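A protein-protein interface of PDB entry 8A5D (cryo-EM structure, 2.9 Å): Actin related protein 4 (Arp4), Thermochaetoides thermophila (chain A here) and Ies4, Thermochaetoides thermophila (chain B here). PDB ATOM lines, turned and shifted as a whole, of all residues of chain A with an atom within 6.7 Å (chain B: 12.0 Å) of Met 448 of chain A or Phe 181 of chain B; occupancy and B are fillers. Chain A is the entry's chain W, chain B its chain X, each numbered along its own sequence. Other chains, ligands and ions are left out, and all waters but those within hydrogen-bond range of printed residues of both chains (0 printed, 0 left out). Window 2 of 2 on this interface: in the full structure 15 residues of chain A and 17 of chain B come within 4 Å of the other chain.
N of Phe 181 of chain B lies within hydrogen-bond range of O of Gln 447 of chain A, 3.1 Å away.
OE2 of Glu 454 of chain A sits at hydrogen-bond distance from OG1 of Thr 182 of chain B, at 3.5 Å.
The indole nitrogen (NE1) of Trp 449 of chain A lies within hydrogen-bond range of a ring nitrogen (ND1) of His 446 of chain A, at 3.3 Å.
NZ of Lys 465 of chain A sits at hydrogen-bond distance from O of Met 448 of chain A.
The side-chain carboxylate (OE1) of Glu 454 of chain A lies within hydrogen-bond range of the side-chain hydroxyl (OG) of Ser 451 of chain A (2.7 Å).
OE2 of Glu 454 of chain A lies within salt-bridge range of NZ of Lys 465 of chain A (2.8 Å).
The backbone carbonyl oxygen of Trp 186 of chain B is in hydrogen-bond range of the backbone NH of Met 178 of chain B (2.9 Å).
OG of Ser 180 of chain B lies within hydrogen-bond range of O of Val 184 of chain B (2.9 Å).
Of the 13 printed residues of chain A, 5 touch a printed residue of chain B.
Printed residues of chain A that touch a printed residue of chain B: Gln 447, Met 448, Trp 449, Ser 451 and Glu 454.
Along chain A the printed residues that touch a printed residue of chain B span positions 447 to 454.
Of the 10 printed residues of chain B, 5 touch a printed residue of chain A.
Hydrophobic or aromatic side chains of chain B within 4 Å of the printed part of chain A: Phe 181 and Trp 186.
Among the printed residues, 7 pairs touch across the chains.
Met 448 of chain A touches one residue of chain B.
Phe 181 of chain B touches just these residues of chain A: Gln 447 (3.1 Å) and Met 448 (3.6 Å).
No residue of chain B comes within 4 Å of Phe 445 of chain A.
Printed residues of chain B within 4 Å of Trp 449 of chain A: Trp 186.
No residue of chain B comes within 4 Å of Ile 450 of chain A.
Printed residues of chain B within 4 Å of Glu 454 of chain A: Thr 182.
Of the printed residues of chain B, Ser 451 of chain A touches Trp 186.
Printed residues of chain A within 4 Å of Thr 182 of chain B: Glu 454 (3.5 Å).
Val 184 of chain B touches none of the printed residues of chain A.
Gly 183 of chain B touches none of the printed residues of chain A.
The nearest printed residue of chain A that does not touch Ser 180 of chain B is Glu 454 of chain A (4.1 Å).
O of Lys 179 of chain B touches CA of Gln 447 of chain A, at 3.8 Å.
CA of Ser 180 of chain B touches O of Gln 447 of chain A (3.3 Å).
Met 448 of chain A touches Phe 181 of chain B.
Trp 449 of chain A touches Trp 186 of chain B (CD1 to CZ2, 3.9 Å).
OG of Ser 451 of chain A touches CD1 of Trp 186 of chain B (3.1 Å).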
ATOM      1  N   PHE A 175       2.431 -12.922 -21.050  1.00  0.00           N
ATOM      2  CA  PHE A 175       1.147 -12.272 -21.421  1.00  0.00           C
ATOM      3  C   PHE A 175       0.656 -12.812 -22.753  1.00  0.00           C
ATOM      4  O   PHE A 175       1.424 -13.261 -23.596  1.00  0.00           O
ATOM      5  CB  PHE A 175       1.391 -10.771 -21.545  1.00  0.00           C
ATOM      6  CG  PHE A 175       0.174  -9.961 -21.879  1.00  0.00           C
ATOM      7  CD1 PHE A 175      -0.894  -9.906 -20.984  1.00  0.00           C
ATOM      8  CD2 PHE A 175       0.089  -9.246 -23.063  1.00  0.00           C
ATOM      9  CE1 PHE A 175      -2.010  -9.128 -21.250  1.00  0.00           C
ATOM     10  CE2 PHE A 175      -1.050  -8.503 -23.349  1.00  0.00           C
ATOM     11  CZ  PHE A 175      -2.097  -8.446 -22.446  1.00  0.00           C
ATOM     12  N   TRP A 176      -0.638 -12.832 -22.911  1.00  0.00           N
ATOM     13  CA  TRP A 176      -1.305 -13.170 -24.187  1.00  0.00           C
ATOM     14  C   TRP A 176      -2.592 -12.368 -24.259  1.00  0.00           C
ATOM     15  O   TRP A 176      -3.220 -12.134 -23.208  1.00  0.00           O
ATOM     16  CB  TRP A 176      -1.561 -14.696 -24.338  1.00  0.00           C
ATOM     17  CG  TRP A 176      -2.052 -15.053 -25.708  1.00  0.00           C
ATOM     18  CD1 TRP A 176      -3.343 -15.212 -26.098  1.00  0.00           C
ATOM     19  CD2 TRP A 176      -1.273 -15.231 -26.896  1.00  0.00           C
ATOM     20  NE1 TRP A 176      -3.424 -15.495 -27.431  1.00  0.00           N
ATOM     21  CE2 TRP A 176      -2.170 -15.467 -27.954  1.00  0.00           C
ATOM     22  CE3 TRP A 176       0.091 -15.222 -27.164  1.00  0.00           C
ATOM     23  CZ2 TRP A 176      -1.747 -15.703 -29.253  1.00  0.00           C
ATOM     24  CZ3 TRP A 176       0.513 -15.408 -28.453  1.00  0.00           C
ATOM     25  CH2 TRP A 176      -0.396 -15.632 -29.483  1.00  0.00           C
ATOM     26  N   THR A 444       0.546 -27.380 -25.934  1.00  0.00           N
ATOM     27  CA  THR A 444       1.061 -26.790 -27.197  1.00  0.00           C
ATOM     28  C   THR A 444       0.993 -25.259 -27.146  1.00  0.00           C
ATOM     29  O   THR A 444       1.710 -24.617 -27.909  1.00  0.00           O
ATOM     30  CB  THR A 444       0.319 -27.391 -28.381  1.00  0.00           C
ATOM     31  OG1 THR A 444       0.598 -28.790 -28.294  1.00  0.00           O
ATOM     32  CG2 THR A 444       0.759 -26.847 -29.722  1.00  0.00           C
ATOM     33  N   PHE A 445       0.186 -24.691 -26.273  1.00  0.00           N
ATOM     34  CA  PHE A 445      -0.049 -23.233 -26.240  1.00  0.00           C
ATOM     35  C   PHE A 445       1.139 -22.570 -25.556  1.00  0.00           C
ATOM     36  O   PHE A 445       1.402 -21.404 -25.854  1.00  0.00           O
ATOM     37  CB  PHE A 445      -1.410 -22.893 -25.604  1.00  0.00           C
ATOM     38  CG  PHE A 445      -1.648 -21.415 -25.497  1.00  0.00           C
ATOM     39  CD1 PHE A 445      -1.912 -20.640 -26.607  1.00  0.00           C
ATOM     40  CD2 PHE A 445      -1.579 -20.778 -24.283  1.00  0.00           C
ATOM     41  CE1 PHE A 445      -2.048 -19.255 -26.514  1.00  0.00           C
ATOM     42  CE2 PHE A 445      -1.705 -19.391 -24.181  1.00  0.00           C
ATOM     43  CZ  PHE A 445      -1.933 -18.630 -25.298  1.00  0.00           C
ATOM     44  N   HIS A 446       1.882 -23.259 -24.689  1.00  0.00           N
ATOM     45  CA  HIS A 446       2.840 -22.548 -23.785  1.00  0.00           C
ATOM     46  C   HIS A 446       4.039 -21.997 -24.558  1.00  0.00           C
ATOM     47  O   HIS A 446       4.721 -21.162 -23.967  1.00  0.00           O
ATOM     48  CB  HIS A 446       3.248 -23.397 -22.560  1.00  0.00           C
ATOM     49  CG  HIS A 446       2.096 -23.844 -21.705  1.00  0.00           C
ATOM     50  ND1 HIS A 446       1.044 -23.005 -21.401  1.00  0.00           N
ATOM     51  CD2 HIS A 446       1.819 -25.026 -21.103  1.00  0.00           C
ATOM     52  CE1 HIS A 446       0.163 -23.631 -20.677  1.00  0.00           C
ATOM     53  NE2 HIS A 446       0.613 -24.889 -20.475  1.00  0.00           N
ATOM     54  N   GLN A 447       4.272 -22.394 -25.825  1.00  0.00           N
ATOM     55  CA  GLN A 447       5.240 -21.705 -26.741  1.00  0.00           C
ATOM     56  C   GLN A 447       4.771 -20.346 -27.282  1.00  0.00           C
ATOM     57  O   GLN A 447       5.603 -19.631 -27.843  1.00  0.00           O
ATOM     58  CB  GLN A 447       5.619 -22.566 -27.919  1.00  0.00           C
ATOM     59  CG  GLN A 447       4.539 -22.799 -28.954  1.00  0.00           C
ATOM     60  CD  GLN A 447       4.817 -24.130 -29.630  1.00  0.00           C
ATOM     61  OE1 GLN A 447       5.973 -24.471 -29.870  1.00  0.00           O
ATOM     62  NE2 GLN A 447       3.793 -24.943 -29.875  1.00  0.00           N
ATOM     63  N   MET A 448       3.540 -19.940 -27.012  1.00  0.00           N
ATOM     64  CA  MET A 448       2.941 -18.723 -27.601  1.00  0.00           C
ATOM     65  C   MET A 448       3.154 -17.509 -26.695  1.00  0.00           C
ATOM     66  O   MET A 448       3.442 -16.431 -27.294  1.00  0.00           O
ATOM     67  CB  MET A 448       1.443 -18.911 -27.868  1.00  0.00           C
ATOM     68  CG  MET A 448       1.077 -20.069 -28.812  1.00  0.00           C
ATOM     69  SD  MET A 448       1.870 -19.953 -30.454  1.00  0.00           S
ATOM     70  CE  MET A 448       1.577 -18.243 -30.888  1.00  0.00           C
ATOM     71  N   TRP A 449       3.088 -17.644 -25.355  1.00  0.00           N
ATOM     72  CA  TRP A 449       3.116 -16.486 -24.405  1.00  0.00           C
ATOM     73  C   TRP A 449       4.209 -15.468 -24.757  1.00  0.00           C
ATOM     74  O   TRP A 449       5.370 -15.885 -24.976  1.00  0.00           O
ATOM     75  CB  TRP A 449       3.386 -16.926 -22.964  1.00  0.00           C
ATOM     76  CG  TRP A 449       2.414 -17.861 -22.322  1.00  0.00           C
ATOM     77  CD1 TRP A 449       2.622 -19.187 -22.109  1.00  0.00           C
ATOM     78  CD2 TRP A 449       1.115 -17.551 -21.770  1.00  0.00           C
ATOM     79  NE1 TRP A 449       1.529 -19.732 -21.504  1.00  0.00           N
ATOM     80  CE2 TRP A 449       0.587 -18.766 -21.309  1.00  0.00           C
ATOM     81  CE3 TRP A 449       0.330 -16.390 -21.650  1.00  0.00           C
ATOM     82  CZ2 TRP A 449      -0.669 -18.847 -20.728  1.00  0.00           C
ATOM     83  CZ3 TRP A 449      -0.924 -16.467 -21.084  1.00  0.00           C
ATOM     84  CH2 TRP A 449      -1.407 -17.686 -20.635  1.00  0.00           C
ATOM     85  N   ILE A 450       3.913 -14.184 -24.711  1.00  0.00           N
ATOM     86  CA  ILE A 450       4.994 -13.182 -24.805  1.00  0.00           C
ATOM     87  C   ILE A 450       5.587 -13.114 -23.417  1.00  0.00           C
ATOM     88  O   ILE A 450       4.901 -12.718 -22.486  1.00  0.00           O
ATOM     89  CB  ILE A 450       4.490 -11.821 -25.284  1.00  0.00           C
ATOM     90  CG1 ILE A 450       4.020 -11.876 -26.731  1.00  0.00           C
ATOM     91  CG2 ILE A 450       5.516 -10.725 -25.078  1.00  0.00           C
ATOM     92  CD1 ILE A 450       3.644 -10.467 -27.173  1.00  0.00           C
ATOM     93  N   SER A 451       6.869 -13.413 -23.316  1.00  0.00           N
ATOM     94  CA  SER A 451       7.687 -13.327 -22.083  1.00  0.00           C
ATOM     95  C   SER A 451       7.884 -11.867 -21.648  1.00  0.00           C
ATOM     96  O   SER A 451       7.872 -10.942 -22.478  1.00  0.00           O
ATOM     97  CB  SER A 451       9.004 -14.008 -22.328  1.00  0.00           C
ATOM     98  OG  SER A 451       8.895 -15.105 -23.248  1.00  0.00           O
ATOM     99  N   GLU A 454      10.949 -10.837 -23.626  1.00  0.00           N
ATOM    100  CA  GLU A 454      10.483 -10.686 -25.034  1.00  0.00           C
ATOM    101  C   GLU A 454       9.855  -9.298 -25.208  1.00  0.00           C
ATOM    102  O   GLU A 454      10.096  -8.667 -26.234  1.00  0.00           O
ATOM    103  CB  GLU A 454       9.539 -11.859 -25.270  1.00  0.00           C
ATOM    104  CG  GLU A 454       9.036 -12.112 -26.671  1.00  0.00           C
ATOM    105  CD  GLU A 454       8.377 -13.516 -26.763  1.00  0.00           C
ATOM    106  OE1 GLU A 454       8.366 -14.275 -25.720  1.00  0.00           O
ATOM    107  OE2 GLU A 454       7.909 -13.897 -27.883  1.00  0.00           O
ATOM    108  N   LYS A 465       3.088 -10.575 -32.990  1.00  0.00           N
ATOM    109  CA  LYS A 465       2.820 -11.887 -32.344  1.00  0.00           C
ATOM    110  C   LYS A 465       1.332 -12.209 -32.275  1.00  0.00           C
ATOM    111  O   LYS A 465       1.097 -13.366 -31.955  1.00  0.00           O
ATOM    112  CB  LYS A 465       3.527 -12.018 -31.000  1.00  0.00           C
ATOM    113  CG  LYS A 465       5.027 -12.301 -31.132  1.00  0.00           C
ATOM    114  CD  LYS A 465       5.697 -13.272 -30.133  1.00  0.00           C
ATOM    115  CE  LYS A 465       4.932 -14.544 -29.769  1.00  0.00           C
ATOM    116  NZ  LYS A 465       5.668 -15.348 -28.772  1.00  0.00           N
ATOM    117  N   ARG A 466       0.411 -11.339 -32.739  1.00  0.00           N
ATOM    118  CA  ARG A 466      -1.018 -11.694 -33.007  1.00  0.00           C
ATOM    119  C   ARG A 466      -1.678 -10.859 -34.108  1.00  0.00           C
ATOM    120  O   ARG A 466      -1.495 -11.215 -35.275  1.00  0.00           O
ATOM    121  CB  ARG A 466      -1.798 -11.462 -31.732  1.00  0.00           C
ATOM    122  CG  ARG A 466      -1.201 -12.295 -30.628  1.00  0.00           C
ATOM    123  CD  ARG A 466      -1.954 -12.147 -29.366  1.00  0.00           C
ATOM    124  NE  ARG A 466      -0.950 -12.516 -28.421  1.00  0.00           N
ATOM    125  CZ  ARG A 466      -0.201 -11.680 -27.750  1.00  0.00           C
ATOM    126  NH1 ARG A 466      -0.404 -10.376 -27.783  1.00  0.00           N
ATOM    127  NH2 ARG A 466       0.717 -12.163 -26.943  1.00  0.00           N
ATOM    128  N   GLN B 177      12.761 -23.638 -16.779  1.00  0.00           N
ATOM    129  CA  GLN B 177      13.071 -22.920 -18.035  1.00  0.00           C
ATOM    130  C   GLN B 177      12.129 -23.431 -19.111  1.00  0.00           C
ATOM    131  O   GLN B 177      12.020 -24.676 -19.283  1.00  0.00           O
ATOM    132  CB  GLN B 177      14.526 -23.135 -18.433  1.00  0.00           C
ATOM    133  CG  GLN B 177      15.476 -22.348 -17.549  1.00  0.00           C
ATOM    134  CD  GLN B 177      16.860 -22.310 -18.146  1.00  0.00           C
ATOM    135  OE1 GLN B 177      17.411 -21.244 -18.409  1.00  0.00           O
ATOM    136  NE2 GLN B 177      17.421 -23.485 -18.389  1.00  0.00           N
ATOM    137  N   MET B 178      11.503 -22.506 -19.835  1.00  0.00           N
ATOM    138  CA  MET B 178      10.650 -22.880 -20.978  1.00  0.00           C
ATOM    139  C   MET B 178      10.777 -21.853 -22.103  1.00  0.00           C
ATOM    140  O   MET B 178      11.347 -20.756 -21.878  1.00  0.00           O
ATOM    141  CB  MET B 178       9.208 -23.067 -20.525  1.00  0.00           C
ATOM    142  CG  MET B 178       8.537 -21.847 -19.994  1.00  0.00           C
ATOM    143  SD  MET B 178       6.775 -22.145 -20.157  1.00  0.00           S
ATOM    144  CE  MET B 178       6.643 -23.607 -19.137  1.00  0.00           C
ATOM    145  N   LYS B 179      10.380 -22.255 -23.307  1.00  0.00           N
ATOM    146  CA  LYS B 179      10.886 -21.623 -24.541  1.00  0.00           C
ATOM    147  C   LYS B 179       9.710 -21.278 -25.443  1.00  0.00           C
ATOM    148  O   LYS B 179       8.890 -22.158 -25.715  1.00  0.00           O
ATOM    149  CB  LYS B 179      11.899 -22.560 -25.200  1.00  0.00           C
ATOM    150  CG  LYS B 179      12.845 -21.894 -26.185  1.00  0.00           C
ATOM    151  CD  LYS B 179      13.816 -22.891 -26.805  1.00  0.00           C
ATOM    152  CE  LYS B 179      14.806 -23.482 -25.818  1.00  0.00           C
ATOM    153  NZ  LYS B 179      15.676 -24.507 -26.448  1.00  0.00           N
ATOM    154  N   SER B 180       9.697 -20.045 -25.937  1.00  0.00           N
ATOM    155  CA  SER B 180       8.796 -19.587 -27.017  1.00  0.00           C
ATOM    156  C   SER B 180       9.225 -20.136 -28.382  1.00  0.00           C
ATOM    157  O   SER B 180      10.396 -20.480 -28.583  1.00  0.00           O
ATOM    158  CB  SER B 180       8.787 -18.103 -27.046  1.00  0.00           C
ATOM    159  OG  SER B 180      10.077 -17.611 -27.317  1.00  0.00           O
ATOM    160  N   PHE B 181       8.316 -20.155 -29.343  1.00  0.00           N
ATOM    161  CA  PHE B 181       8.604 -20.667 -30.705  1.00  0.00           C
ATOM    162  C   PHE B 181       9.575 -19.717 -31.419  1.00  0.00           C
ATOM    163  O   PHE B 181      10.183 -20.154 -32.383  1.00  0.00           O
ATOM    164  CB  PHE B 181       7.292 -20.946 -31.441  1.00  0.00           C
ATOM    165  CG  PHE B 181       6.626 -19.747 -32.036  1.00  0.00           C
ATOM    166  CD1 PHE B 181       5.600 -19.112 -31.379  1.00  0.00           C
ATOM    167  CD2 PHE B 181       6.995 -19.296 -33.291  1.00  0.00           C
ATOM    168  CE1 PHE B 181       4.973 -18.023 -31.957  1.00  0.00           C
ATOM    169  CE2 PHE B 181       6.368 -18.207 -33.868  1.00  0.00           C
ATOM    170  CZ  PHE B 181       5.365 -17.567 -33.195  1.00  0.00           C
ATOM    171  N   THR B 182       9.707 -18.467 -30.981  1.00  0.00           N
ATOM    172  CA  THR B 182      10.716 -17.500 -31.493  1.00  0.00           C
ATOM    173  C   THR B 182      12.054 -17.581 -30.715  1.00  0.00           C
ATOM    174  O   THR B 182      12.911 -16.642 -30.829  1.00  0.00           O
ATOM    175  CB  THR B 182      10.142 -16.080 -31.465  1.00  0.00           C
ATOM    176  OG1 THR B 182       9.866 -15.680 -30.117  1.00  0.00           O
ATOM    177  CG2 THR B 182       8.881 -15.982 -32.298  1.00  0.00           C
ATOM    178  N   GLY B 183      12.241 -18.624 -29.911  1.00  0.00           N
ATOM    179  CA  GLY B 183      13.534 -18.964 -29.299  1.00  0.00           C
ATOM    180  C   GLY B 183      13.851 -18.231 -28.006  1.00  0.00           C
ATOM    181  O   GLY B 183      14.921 -18.537 -27.434  1.00  0.00           O
ATOM    182  N   VAL B 184      12.995 -17.319 -27.531  1.00  0.00           N
ATOM    183  CA  VAL B 184      13.220 -16.605 -26.234  1.00  0.00           C
ATOM    184  C   VAL B 184      12.889 -17.550 -25.071  1.00  0.00           C
ATOM    185  O   VAL B 184      11.830 -18.206 -25.123  1.00  0.00           O
ATOM    186  CB  VAL B 184      12.434 -15.296 -26.116  1.00  0.00           C
ATOM    187  CG1 VAL B 184      12.803 -14.578 -24.837  1.00  0.00           C
ATOM    188  CG2 VAL B 184      12.682 -14.390 -27.308  1.00  0.00           C
ATOM    189  N   VAL B 185      13.794 -17.600 -24.081  1.00  0.00           N
ATOM    190  CA  VAL B 185      13.742 -18.503 -22.893  1.00  0.00           C
ATOM    191  C   VAL B 185      13.331 -17.707 -21.663  1.00  0.00           C
ATOM    192  O   VAL B 185      13.908 -16.617 -21.428  1.00  0.00           O
ATOM    193  CB  VAL B 185      15.084 -19.208 -22.651  1.00  0.00           C
ATOM    194  CG1 VAL B 185      15.094 -19.954 -21.325  1.00  0.00           C
ATOM    195  CG2 VAL B 185      15.417 -20.158 -23.794  1.00  0.00           C
ATOM    196  N   TRP B 186      12.376 -18.243 -20.896  1.00  0.00           N
ATOM    197  CA  TRP B 186      11.882 -17.580 -19.664  1.00  0.00           C
ATOM    198  C   TRP B 186      11.581 -18.600 -18.570  1.00  0.00           C
ATOM    199  O   TRP B 186      11.541 -19.803 -18.863  1.00  0.00           O
ATOM    200  CB  TRP B 186      10.687 -16.685 -19.998  1.00  0.00           C
ATOM    201  CG  TRP B 186       9.490 -17.376 -20.570  1.00  0.00           C
ATOM    202  CD1 TRP B 186       9.333 -17.783 -21.853  1.00  0.00           C
ATOM    203  CD2 TRP B 186       8.262 -17.710 -19.896  1.00  0.00           C
ATOM    204  NE1 TRP B 186       8.119 -18.390 -22.020  1.00  0.00           N
ATOM    205  CE2 TRP B 186       7.434 -18.363 -20.838  1.00  0.00           C
ATOM    206  CE3 TRP B 186       7.798 -17.589 -18.582  1.00  0.00           C
ATOM    207  CZ2 TRP B 186       6.150 -18.823 -20.534  1.00  0.00           C
ATOM    208  CZ3 TRP B 186       6.535 -18.060 -18.279  1.00  0.00           C
ATOM    209  CH2 TRP B 186       5.721 -18.667 -19.241  1.00  0.00           C
